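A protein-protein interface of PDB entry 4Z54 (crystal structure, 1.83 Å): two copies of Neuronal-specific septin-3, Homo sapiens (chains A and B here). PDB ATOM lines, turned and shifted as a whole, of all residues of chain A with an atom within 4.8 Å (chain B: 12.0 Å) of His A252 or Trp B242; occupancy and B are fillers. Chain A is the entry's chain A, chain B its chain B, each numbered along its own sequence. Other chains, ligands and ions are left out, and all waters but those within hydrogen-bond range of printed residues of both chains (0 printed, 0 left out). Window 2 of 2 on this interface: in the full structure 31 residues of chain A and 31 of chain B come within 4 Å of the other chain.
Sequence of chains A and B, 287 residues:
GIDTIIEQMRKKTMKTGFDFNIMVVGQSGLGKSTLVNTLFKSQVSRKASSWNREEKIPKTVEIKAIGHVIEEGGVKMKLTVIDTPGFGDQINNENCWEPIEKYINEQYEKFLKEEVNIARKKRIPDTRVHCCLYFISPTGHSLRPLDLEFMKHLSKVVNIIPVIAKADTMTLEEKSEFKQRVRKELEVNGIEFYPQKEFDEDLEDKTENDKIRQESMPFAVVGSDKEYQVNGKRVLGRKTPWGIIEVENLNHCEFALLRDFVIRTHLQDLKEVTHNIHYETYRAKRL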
ATOM      1  N   LYS A 175     -13.825   2.781 -18.590  1.00  0.00           N
ATOM      2  CA  LYS A 175     -14.666   1.731 -18.017  1.00  0.00           C
ATOM      3  C   LYS A 175     -15.964   1.572 -18.809  1.00  0.00           C
ATOM      4  O   LYS A 175     -16.388   0.455 -19.116  1.00  0.00           O
ATOM      5  CB  LYS A 175     -14.955   2.051 -16.543  1.00  0.00           C
ATOM      6  CG  LYS A 175     -15.946   1.159 -15.833  1.00  0.00           C
ATOM      7  CD  LYS A 175     -16.112   1.611 -14.365  1.00  0.00           C
ATOM      8  CE  LYS A 175     -17.429   1.127 -13.744  1.00  0.00           C
ATOM      9  NZ  LYS A 175     -17.500   1.332 -12.252  1.00  0.00           N
ATOM     10  N   TRP A 242      -3.141   8.349  -3.605  1.00  0.00           N
ATOM     11  CA  TRP A 242      -4.092   9.450  -3.763  1.00  0.00           C
ATOM     12  C   TRP A 242      -5.306   9.330  -2.852  1.00  0.00           C
ATOM     13  O   TRP A 242      -5.920  10.339  -2.486  1.00  0.00           O
ATOM     14  CB  TRP A 242      -4.548   9.558  -5.215  1.00  0.00           C
ATOM     15  CG  TRP A 242      -3.451  10.060  -6.095  1.00  0.00           C
ATOM     16  CD1 TRP A 242      -3.233  11.349  -6.490  1.00  0.00           C
ATOM     17  CD2 TRP A 242      -2.392   9.281  -6.654  1.00  0.00           C
ATOM     18  NE1 TRP A 242      -2.106  11.416  -7.274  1.00  0.00           N
ATOM     19  CE2 TRP A 242      -1.572  10.159  -7.391  1.00  0.00           C
ATOM     20  CE3 TRP A 242      -2.059   7.924  -6.612  1.00  0.00           C
ATOM     21  CZ2 TRP A 242      -0.444   9.719  -8.078  1.00  0.00           C
ATOM     22  CZ3 TRP A 242      -0.942   7.490  -7.294  1.00  0.00           C
ATOM     23  CH2 TRP A 242      -0.146   8.383  -8.014  1.00  0.00           C
ATOM     24  N   GLY A 243      -5.664   8.106  -2.486  1.00  0.00           N
ATOM     25  CA  GLY A 243      -6.735   7.931  -1.529  1.00  0.00           C
ATOM     26  C   GLY A 243      -7.232   6.508  -1.387  1.00  0.00           C
ATOM     27  O   GLY A 243      -6.677   5.578  -1.976  1.00  0.00           O
ATOM     28  N   ILE A 244      -8.291   6.356  -0.602  1.00  0.00           N
ATOM     29  CA  ILE A 244      -8.902   5.055  -0.360  1.00  0.00           C
ATOM     30  C   ILE A 244      -9.997   4.801  -1.370  1.00  0.00           C
ATOM     31  O   ILE A 244     -10.970   5.557  -1.458  1.00  0.00           O
ATOM     32  CB  ILE A 244      -9.508   4.953   1.050  1.00  0.00           C
ATOM     33  CG1 ILE A 244      -8.460   5.272   2.113  1.00  0.00           C
ATOM     34  CG2 ILE A 244     -10.147   3.576   1.262  1.00  0.00           C
ATOM     35  CD1 ILE A 244      -7.377   4.268   2.198  1.00  0.00           C
ATOM     36  N   ILE A 245      -9.833   3.738  -2.145  1.00  0.00           N
ATOM     37  CA  ILE A 245     -10.875   3.298  -3.047  1.00  0.00           C
ATOM     38  C   ILE A 245     -11.765   2.378  -2.257  1.00  0.00           C
ATOM     39  O   ILE A 245     -11.290   1.369  -1.763  1.00  0.00           O
ATOM     40  CB  ILE A 245     -10.302   2.546  -4.260  1.00  0.00           C
ATOM     41  CG1 ILE A 245      -9.277   3.419  -4.979  1.00  0.00           C
ATOM     42  CG2 ILE A 245     -11.431   2.094  -5.178  1.00  0.00           C
ATOM     43  CD1 ILE A 245      -8.459   2.680  -6.021  1.00  0.00           C
ATOM     44  N   GLU A 246     -13.033   2.735  -2.097  1.00  0.00           N
ATOM     45  CA  GLU A 246     -13.904   1.992  -1.195  1.00  0.00           C
ATOM     46  C   GLU A 246     -14.670   0.929  -1.960  1.00  0.00           C
ATOM     47  O   GLU A 246     -15.466   1.237  -2.835  1.00  0.00           O
ATOM     48  CB  GLU A 246     -14.867   2.934  -0.484  1.00  0.00           C
ATOM     49  CG  GLU A 246     -14.184   4.013   0.315  1.00  0.00           C
ATOM     50  CD  GLU A 246     -15.138   5.112   0.683  1.00  0.00           C
ATOM     51  OE1 GLU A 246     -16.327   4.793   0.909  1.00  0.00           O
ATOM     52  OE2 GLU A 246     -14.712   6.289   0.722  1.00  0.00           O
ATOM     53  N   ASN A 249     -18.565   1.069  -1.920  1.00  0.00           N
ATOM     54  CA  ASN A 249     -19.135   2.356  -2.295  1.00  0.00           C
ATOM     55  C   ASN A 249     -19.457   2.352  -3.797  1.00  0.00           C
ATOM     56  O   ASN A 249     -18.559   2.207  -4.627  1.00  0.00           O
ATOM     57  CB  ASN A 249     -18.149   3.475  -1.927  1.00  0.00           C
ATOM     58  CG  ASN A 249     -18.729   4.856  -2.094  1.00  0.00           C
ATOM     59  OD1 ASN A 249     -19.605   5.080  -2.921  1.00  0.00           O
ATOM     60  ND2 ASN A 249     -18.215   5.803  -1.318  1.00  0.00           N
ATOM     61  N   LEU A 250     -20.737   2.504  -4.133  1.00  0.00           N
ATOM     62  CA  LEU A 250     -21.202   2.468  -5.521  1.00  0.00           C
ATOM     63  C   LEU A 250     -20.620   3.591  -6.391  1.00  0.00           C
ATOM     64  O   LEU A 250     -20.622   3.506  -7.624  1.00  0.00           O
ATOM     65  CB  LEU A 250     -22.728   2.539  -5.556  1.00  0.00           C
ATOM     66  CG  LEU A 250     -23.451   1.349  -4.923  1.00  0.00           C
ATOM     67  CD1 LEU A 250     -24.961   1.601  -4.820  1.00  0.00           C
ATOM     68  CD2 LEU A 250     -23.161   0.079  -5.713  1.00  0.00           C
ATOM     69  N   ASN A 251     -20.143   4.651  -5.750  1.00  0.00           N
ATOM     70  CA  ASN A 251     -19.507   5.747  -6.465  1.00  0.00           C
ATOM     71  C   ASN A 251     -18.083   5.392  -6.876  1.00  0.00           C
ATOM     72  O   ASN A 251     -17.491   6.068  -7.723  1.00  0.00           O
ATOM     73  CB  ASN A 251     -19.492   7.020  -5.609  1.00  0.00           C
ATOM     74  CG  ASN A 251     -20.885   7.485  -5.224  1.00  0.00           C
ATOM     75  OD1 ASN A 251     -21.843   7.324  -5.982  1.00  0.00           O
ATOM     76  ND2 ASN A 251     -21.003   8.069  -4.039  1.00  0.00           N
ATOM     77  N   HIS A 252     -17.528   4.353  -6.254  1.00  0.00           N
ATOM     78  CA  HIS A 252     -16.150   3.948  -6.515  1.00  0.00           C
ATOM     79  C   HIS A 252     -16.051   2.712  -7.413  1.00  0.00           C
ATOM     80  O   HIS A 252     -15.215   2.669  -8.317  1.00  0.00           O
ATOM     81  CB  HIS A 252     -15.418   3.697  -5.199  1.00  0.00           C
ATOM     82  CG  HIS A 252     -15.174   4.930  -4.384  1.00  0.00           C
ATOM     83  ND1 HIS A 252     -14.246   4.981  -3.370  1.00  0.00           N
ATOM     84  CD2 HIS A 252     -15.735   6.168  -4.434  1.00  0.00           C
ATOM     85  CE1 HIS A 252     -14.240   6.185  -2.826  1.00  0.00           C
ATOM     86  NE2 HIS A 252     -15.132   6.926  -3.459  1.00  0.00           N
ATOM     87  N   CYS A 253     -16.894   1.708  -7.169  1.00  0.00           N
ATOM     88  CA  CYS A 253     -16.939   0.531  -8.044  1.00  0.00           C
ATOM     89  C   CYS A 253     -18.255  -0.214  -7.910  1.00  0.00           C
ATOM     90  O   CYS A 253     -19.146   0.218  -7.179  1.00  0.00           O
ATOM     91  CB  CYS A 253     -15.792  -0.434  -7.742  1.00  0.00           C
ATOM     92  SG  CYS A 253     -15.986  -1.322  -6.204  1.00  0.00           S
ATOM     93  N   ASP B 168       0.372   2.416 -11.825  1.00  0.00           N
ATOM     94  CA  ASP B 168      -0.637   2.982 -10.943  1.00  0.00           C
ATOM     95  C   ASP B 168      -1.624   1.919 -10.444  1.00  0.00           C
ATOM     96  O   ASP B 168      -2.437   2.192  -9.561  1.00  0.00           O
ATOM     97  CB  ASP B 168      -1.400   4.107 -11.651  1.00  0.00           C
ATOM     98  CG  ASP B 168      -1.988   3.663 -12.992  1.00  0.00           C
ATOM     99  OD1 ASP B 168      -1.226   3.141 -13.831  1.00  0.00           O
ATOM    100  OD2 ASP B 168      -3.213   3.838 -13.205  1.00  0.00           O
ATOM    101  N   THR B 169      -1.555   0.732 -11.028  1.00  0.00           N
ATOM    102  CA  THR B 169      -2.277  -0.469 -10.580  1.00  0.00           C
ATOM    103  C   THR B 169      -1.906  -0.872  -9.155  1.00  0.00           C
ATOM    104  O   THR B 169      -2.711  -1.442  -8.423  1.00  0.00           O
ATOM    105  CB  THR B 169      -1.966  -1.668 -11.522  1.00  0.00           C
ATOM    106  OG1 THR B 169      -2.440  -1.374 -12.832  1.00  0.00           O
ATOM    107  CG2 THR B 169      -2.600  -2.979 -11.035  1.00  0.00           C
ATOM    108  N   MET B 170      -0.677  -0.559  -8.766  1.00  0.00           N
ATOM    109  CA  MET B 170      -0.108  -1.086  -7.528  1.00  0.00           C
ATOM    110  C   MET B 170      -0.044  -0.068  -6.400  1.00  0.00           C
ATOM    111  O   MET B 170       0.236   1.098  -6.631  1.00  0.00           O
ATOM    112  CB  MET B 170       1.299  -1.616  -7.803  1.00  0.00           C
ATOM    113  CG  MET B 170       1.326  -2.783  -8.771  1.00  0.00           C
ATOM    114  SD  MET B 170       3.021  -3.270  -9.187  1.00  0.00           S
ATOM    115  CE  MET B 170       3.557  -1.867 -10.157  1.00  0.00           C
ATOM    116  N   THR B 171      -0.278  -0.520  -5.174  1.00  0.00           N
ATOM    117  CA  THR B 171       0.066   0.284  -4.014  1.00  0.00           C
ATOM    118  C   THR B 171       1.584   0.398  -3.929  1.00  0.00           C
ATOM    119  O   THR B 171       2.310  -0.315  -4.637  1.00  0.00           O
ATOM    120  CB  THR B 171      -0.454  -0.319  -2.707  1.00  0.00           C
ATOM    121  OG1 THR B 171       0.214  -1.565  -2.479  1.00  0.00           O
ATOM    122  CG2 THR B 171      -1.968  -0.520  -2.762  1.00  0.00           C
ATOM    123  N   TYR B 228      -2.443  18.169 -18.278  1.00  0.00           N
ATOM    124  CA  TYR B 228      -3.262  18.827 -17.263  1.00  0.00           C
ATOM    125  C   TYR B 228      -2.446  19.906 -16.590  1.00  0.00           C
ATOM    126  O   TYR B 228      -1.212  19.836 -16.573  1.00  0.00           O
ATOM    127  CB  TYR B 228      -3.759  17.813 -16.238  1.00  0.00           C
ATOM    128  CG  TYR B 228      -4.648  16.761 -16.846  1.00  0.00           C
ATOM    129  CD1 TYR B 228      -6.004  16.997 -17.021  1.00  0.00           C
ATOM    130  CD2 TYR B 228      -4.133  15.538 -17.261  1.00  0.00           C
ATOM    131  CE1 TYR B 228      -6.829  16.045 -17.581  1.00  0.00           C
ATOM    132  CE2 TYR B 228      -4.951  14.577 -17.826  1.00  0.00           C
ATOM    133  CZ  TYR B 228      -6.299  14.835 -17.984  1.00  0.00           C
ATOM    134  OH  TYR B 228      -7.126  13.889 -18.546  1.00  0.00           O
ATOM    135  N   VAL B 230      -1.060  21.272 -13.437  1.00  0.00           N
ATOM    136  CA  VAL B 230      -0.758  20.959 -12.051  1.00  0.00           C
ATOM    137  C   VAL B 230       0.272  21.958 -11.550  1.00  0.00           C
ATOM    138  O   VAL B 230       1.318  22.142 -12.178  1.00  0.00           O
ATOM    139  CB  VAL B 230      -0.220  19.532 -11.891  1.00  0.00           C
ATOM    140  CG1 VAL B 230      -0.023  19.206 -10.415  1.00  0.00           C
ATOM    141  CG2 VAL B 230      -1.160  18.537 -12.544  1.00  0.00           C
ATOM    142  N   GLY B 237      -0.240  13.805 -17.670  1.00  0.00           N
ATOM    143  CA  GLY B 237      -0.879  13.221 -16.512  1.00  0.00           C
ATOM    144  C   GLY B 237      -2.033  12.318 -16.841  1.00  0.00           C
ATOM    145  O   GLY B 237      -2.659  12.418 -17.903  1.00  0.00           O
ATOM    146  N   ARG B 238      -2.333  11.450 -15.892  1.00  0.00           N
ATOM    147  CA  ARG B 238      -3.428  10.528 -16.048  1.00  0.00           C
ATOM    148  C   ARG B 238      -4.475  10.854 -15.011  1.00  0.00           C
ATOM    149  O   ARG B 238      -4.234  10.729 -13.807  1.00  0.00           O
ATOM    150  CB  ARG B 238      -2.932   9.087 -15.918  1.00  0.00           C
ATOM    151  CG  ARG B 238      -4.004   8.074 -16.162  1.00  0.00           C
ATOM    152  CD  ARG B 238      -3.444   6.666 -16.316  1.00  0.00           C
ATOM    153  NE  ARG B 238      -4.540   5.753 -16.043  1.00  0.00           N
ATOM    154  CZ  ARG B 238      -5.436   5.407 -16.951  1.00  0.00           C
ATOM    155  NH1 ARG B 238      -5.312   5.847 -18.206  1.00  0.00           N
ATOM    156  NH2 ARG B 238      -6.438   4.614 -16.605  1.00  0.00           N
ATOM    157  N   LYS B 239      -5.629  11.308 -15.480  1.00  0.00           N
ATOM    158  CA  LYS B 239      -6.679  11.737 -14.585  1.00  0.00           C
ATOM    159  C   LYS B 239      -7.571  10.565 -14.265  1.00  0.00           C
ATOM    160  O   LYS B 239      -8.381  10.147 -15.082  1.00  0.00           O
ATOM    161  CB  LYS B 239      -7.506  12.873 -15.183  1.00  0.00           C
ATOM    162  CG  LYS B 239      -8.577  13.392 -14.219  1.00  0.00           C
ATOM    163  CD  LYS B 239      -9.422  14.480 -14.834  1.00  0.00           C
ATOM    164  CE  LYS B 239     -10.492  14.926 -13.854  1.00  0.00           C
ATOM    165  NZ  LYS B 239     -11.557  15.724 -14.517  1.00  0.00           N
ATOM    166  N   THR B 240      -7.394  10.038 -13.066  1.00  0.00           N
ATOM    167  CA  THR B 240      -8.221   8.962 -12.563  1.00  0.00           C
ATOM    168  C   THR B 240      -9.362   9.573 -11.785  1.00  0.00           C
ATOM    169  O   THR B 240      -9.327  10.767 -11.470  1.00  0.00           O
ATOM    170  CB  THR B 240      -7.415   8.016 -11.661  1.00  0.00           C
ATOM    171  OG1 THR B 240      -7.194   8.645 -10.393  1.00  0.00           O
ATOM    172  CG2 THR B 240      -6.079   7.684 -12.316  1.00  0.00           C
ATOM    173  N   PRO B 241     -10.382   8.768 -11.446  1.00  0.00           N
ATOM    174  CA  PRO B 241     -11.432   9.359 -10.609  1.00  0.00           C
ATOM    175  C   PRO B 241     -10.979   9.740  -9.188  1.00  0.00           C
ATOM    176  O   PRO B 241     -11.807  10.169  -8.393  1.00  0.00           O
ATOM    177  CB  PRO B 241     -12.507   8.258 -10.558  1.00  0.00           C
ATOM    178  CG  PRO B 241     -11.839   7.015 -11.043  1.00  0.00           C
ATOM    179  CD  PRO B 241     -10.779   7.456 -11.989  1.00  0.00           C
ATOM    180  N   TRP B 242      -9.693   9.584  -8.883  1.00  0.00           N
ATOM    181  CA  TRP B 242      -9.192   9.901  -7.550  1.00  0.00           C
ATOM    182  C   TRP B 242      -8.130  10.994  -7.532  1.00  0.00           C
ATOM    183  O   TRP B 242      -7.728  11.456  -6.464  1.00  0.00           O
ATOM    184  CB  TRP B 242      -8.638   8.643  -6.880  1.00  0.00           C
ATOM    185  CG  TRP B 242      -9.556   8.129  -5.824  1.00  0.00           C
ATOM    186  CD1 TRP B 242     -10.264   6.963  -5.845  1.00  0.00           C
ATOM    187  CD2 TRP B 242      -9.899   8.785  -4.597  1.00  0.00           C
ATOM    188  NE1 TRP B 242     -11.014   6.847  -4.699  1.00  0.00           N
ATOM    189  CE2 TRP B 242     -10.807   7.953  -3.917  1.00  0.00           C
ATOM    190  CE3 TRP B 242      -9.516   9.993  -4.005  1.00  0.00           C
ATOM    191  CZ2 TRP B 242     -11.342   8.291  -2.678  1.00  0.00           C
ATOM    192  CZ3 TRP B 242     -10.048  10.324  -2.772  1.00  0.00           C
ATOM    193  CH2 TRP B 242     -10.950   9.476  -2.122  1.00  0.00           C
ATOM    194  N   GLY B 243      -7.679  11.407  -8.711  1.00  0.00           N
ATOM    195  CA  GLY B 243      -6.704  12.479  -8.812  1.00  0.00           C
ATOM    196  C   GLY B 243      -5.924  12.435 -10.105  1.00  0.00           C
ATOM    197  O   GLY B 243      -6.116  11.518 -10.909  1.00  0.00           O
ATOM    198  N   ILE B 244      -5.045  13.415 -10.309  1.00  0.00           N
ATOM    199  CA  ILE B 244      -4.168  13.421 -11.493  1.00  0.00           C
ATOM    200  C   ILE B 244      -2.799  12.834 -11.190  1.00  0.00           C
ATOM    201  O   ILE B 244      -2.034  13.399 -10.410  1.00  0.00           O
ATOM    202  CB  ILE B 244      -3.967  14.841 -12.056  1.00  0.00           C
ATOM    203  CG1 ILE B 244      -5.269  15.382 -12.627  1.00  0.00           C
ATOM    204  CG2 ILE B 244      -2.899  14.830 -13.158  1.00  0.00           C
ATOM    205  CD1 ILE B 244      -5.230  16.868 -12.866  1.00  0.00           C
ATOM    206  N   ILE B 245      -2.485  11.706 -11.820  1.00  0.00           N
ATOM    207  CA  ILE B 245      -1.170  11.104 -11.698  1.00  0.00           C
ATOM    208  C   ILE B 245      -0.209  11.785 -12.668  1.00  0.00           C
ATOM    209  O   ILE B 245      -0.415  11.728 -13.873  1.00  0.00           O
ATOM    210  CB  ILE B 245      -1.214   9.585 -11.993  1.00  0.00           C
ATOM    211  CG1 ILE B 245      -2.269   8.911 -11.117  1.00  0.00           C
ATOM    212  CG2 ILE B 245       0.164   8.960 -11.799  1.00  0.00           C
ATOM    213  CD1 ILE B 245      -2.578   7.485 -11.520  1.00  0.00           C
ATOM    214  N   GLU B 246       0.818  12.446 -12.139  1.00  0.00           N
ATOM    215  CA  GLU B 246       1.779  13.184 -12.959  1.00  0.00           C
ATOM    216  C   GLU B 246       2.882  12.245 -13.454  1.00  0.00           C
ATOM    217  O   GLU B 246       3.716  11.770 -12.678  1.00  0.00           O
ATOM    218  CB  GLU B 246       2.377  14.355 -12.168  1.00  0.00           C
ATOM    219  CG  GLU B 246       1.339  15.221 -11.453  1.00  0.00           C
ATOM    220  CD  GLU B 246       1.946  16.089 -10.364  1.00  0.00           C
ATOM    221  OE1 GLU B 246       3.082  16.587 -10.552  1.00  0.00           O
ATOM    222  OE2 GLU B 246       1.287  16.268  -9.314  1.00  0.00           O
ATOM    223  N   HIS B 252       5.448  10.118  -8.168  1.00  0.00           N
ATOM    224  CA  HIS B 252       4.224   9.459  -8.643  1.00  0.00           C
ATOM    225  C   HIS B 252       4.478   8.168  -9.426  1.00  0.00           C
ATOM    226  O   HIS B 252       3.717   7.207  -9.310  1.00  0.00           O
ATOM    227  CB  HIS B 252       3.420  10.408  -9.528  1.00  0.00           C
ATOM    228  CG  HIS B 252       2.722  11.498  -8.778  1.00  0.00           C
ATOM    229  ND1 HIS B 252       1.650  12.186  -9.305  1.00  0.00           N
ATOM    230  CD2 HIS B 252       2.958  12.041  -7.562  1.00  0.00           C
ATOM    231  CE1 HIS B 252       1.245  13.095  -8.435  1.00  0.00           C
ATOM    232  NE2 HIS B 252       2.020  13.029  -7.370  1.00  0.00           N
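NE1 of Trp B242 lies close to O of Ile A244.
The backbone NH (N) of Glu A246 is in hydrogen-bond range of a ring nitrogen (ND1) of His A252.
The backbone NH (N) of Arg B238 sits at hydrogen-bond distance from the backbone carbonyl oxygen (O) of Ile B245 (2.8 Å).
N of Glu B246 sits at hydrogen-bond distance from ND1 of His B252, 3.0 Å away.
The side-chain hydroxyl of Thr B240 sits close to the backbone NH of Trp B242 (3.1 Å).
Among the printed residues, merely in contact across the chains: Trp A242 with Trp B242, Trp A242 with Ile B244, Trp A242 with Ile B245, Trp A242 with His B252, Ile A245 with Trp B242 and His A252 with Trp B242.
Printed residues of chain A within 4 Å of Trp B242: Trp A242, Ile A244, Ile A245 and His A252.
Asn A249 touches none of the printed residues of chain B.
No residue of chain B comes within 4 Å of Cys A253.
Of the printed residues of chain A, Ile B244 touches Trp A242 (3.7 Å).
Printed residues of chain B within 4 Å of Ile A245: Trp B242 (3.8 Å).
The nearest printed residue of chain A that does not touch Trp B242 is Gly A243 (4.3 Å).
Hydrophobic or aromatic side chains of chain A within 4 Å of the printed part of chain B: Trp A242, Ile A245 and His A252.
Hydrophobic or aromatic side chains of chain B within 4 Å of the printed part of chain A: Trp B242, Ile B245 and His B252.
Among the printed residues, 7 pairs touch across the chains.
Trp B242 touches its own counterpart, Trp A242.
Trp A242 touches Ile B244, and with the chains exchanged Ile A244 touches Trp B242.
Trp A242 touches Ile B245, and with the chains exchanged Ile A245 touches Trp B242.
Trp A242 touches His B252, and with the chains exchanged His A252 touches Trp B242.
6 positions are printed for both chains.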
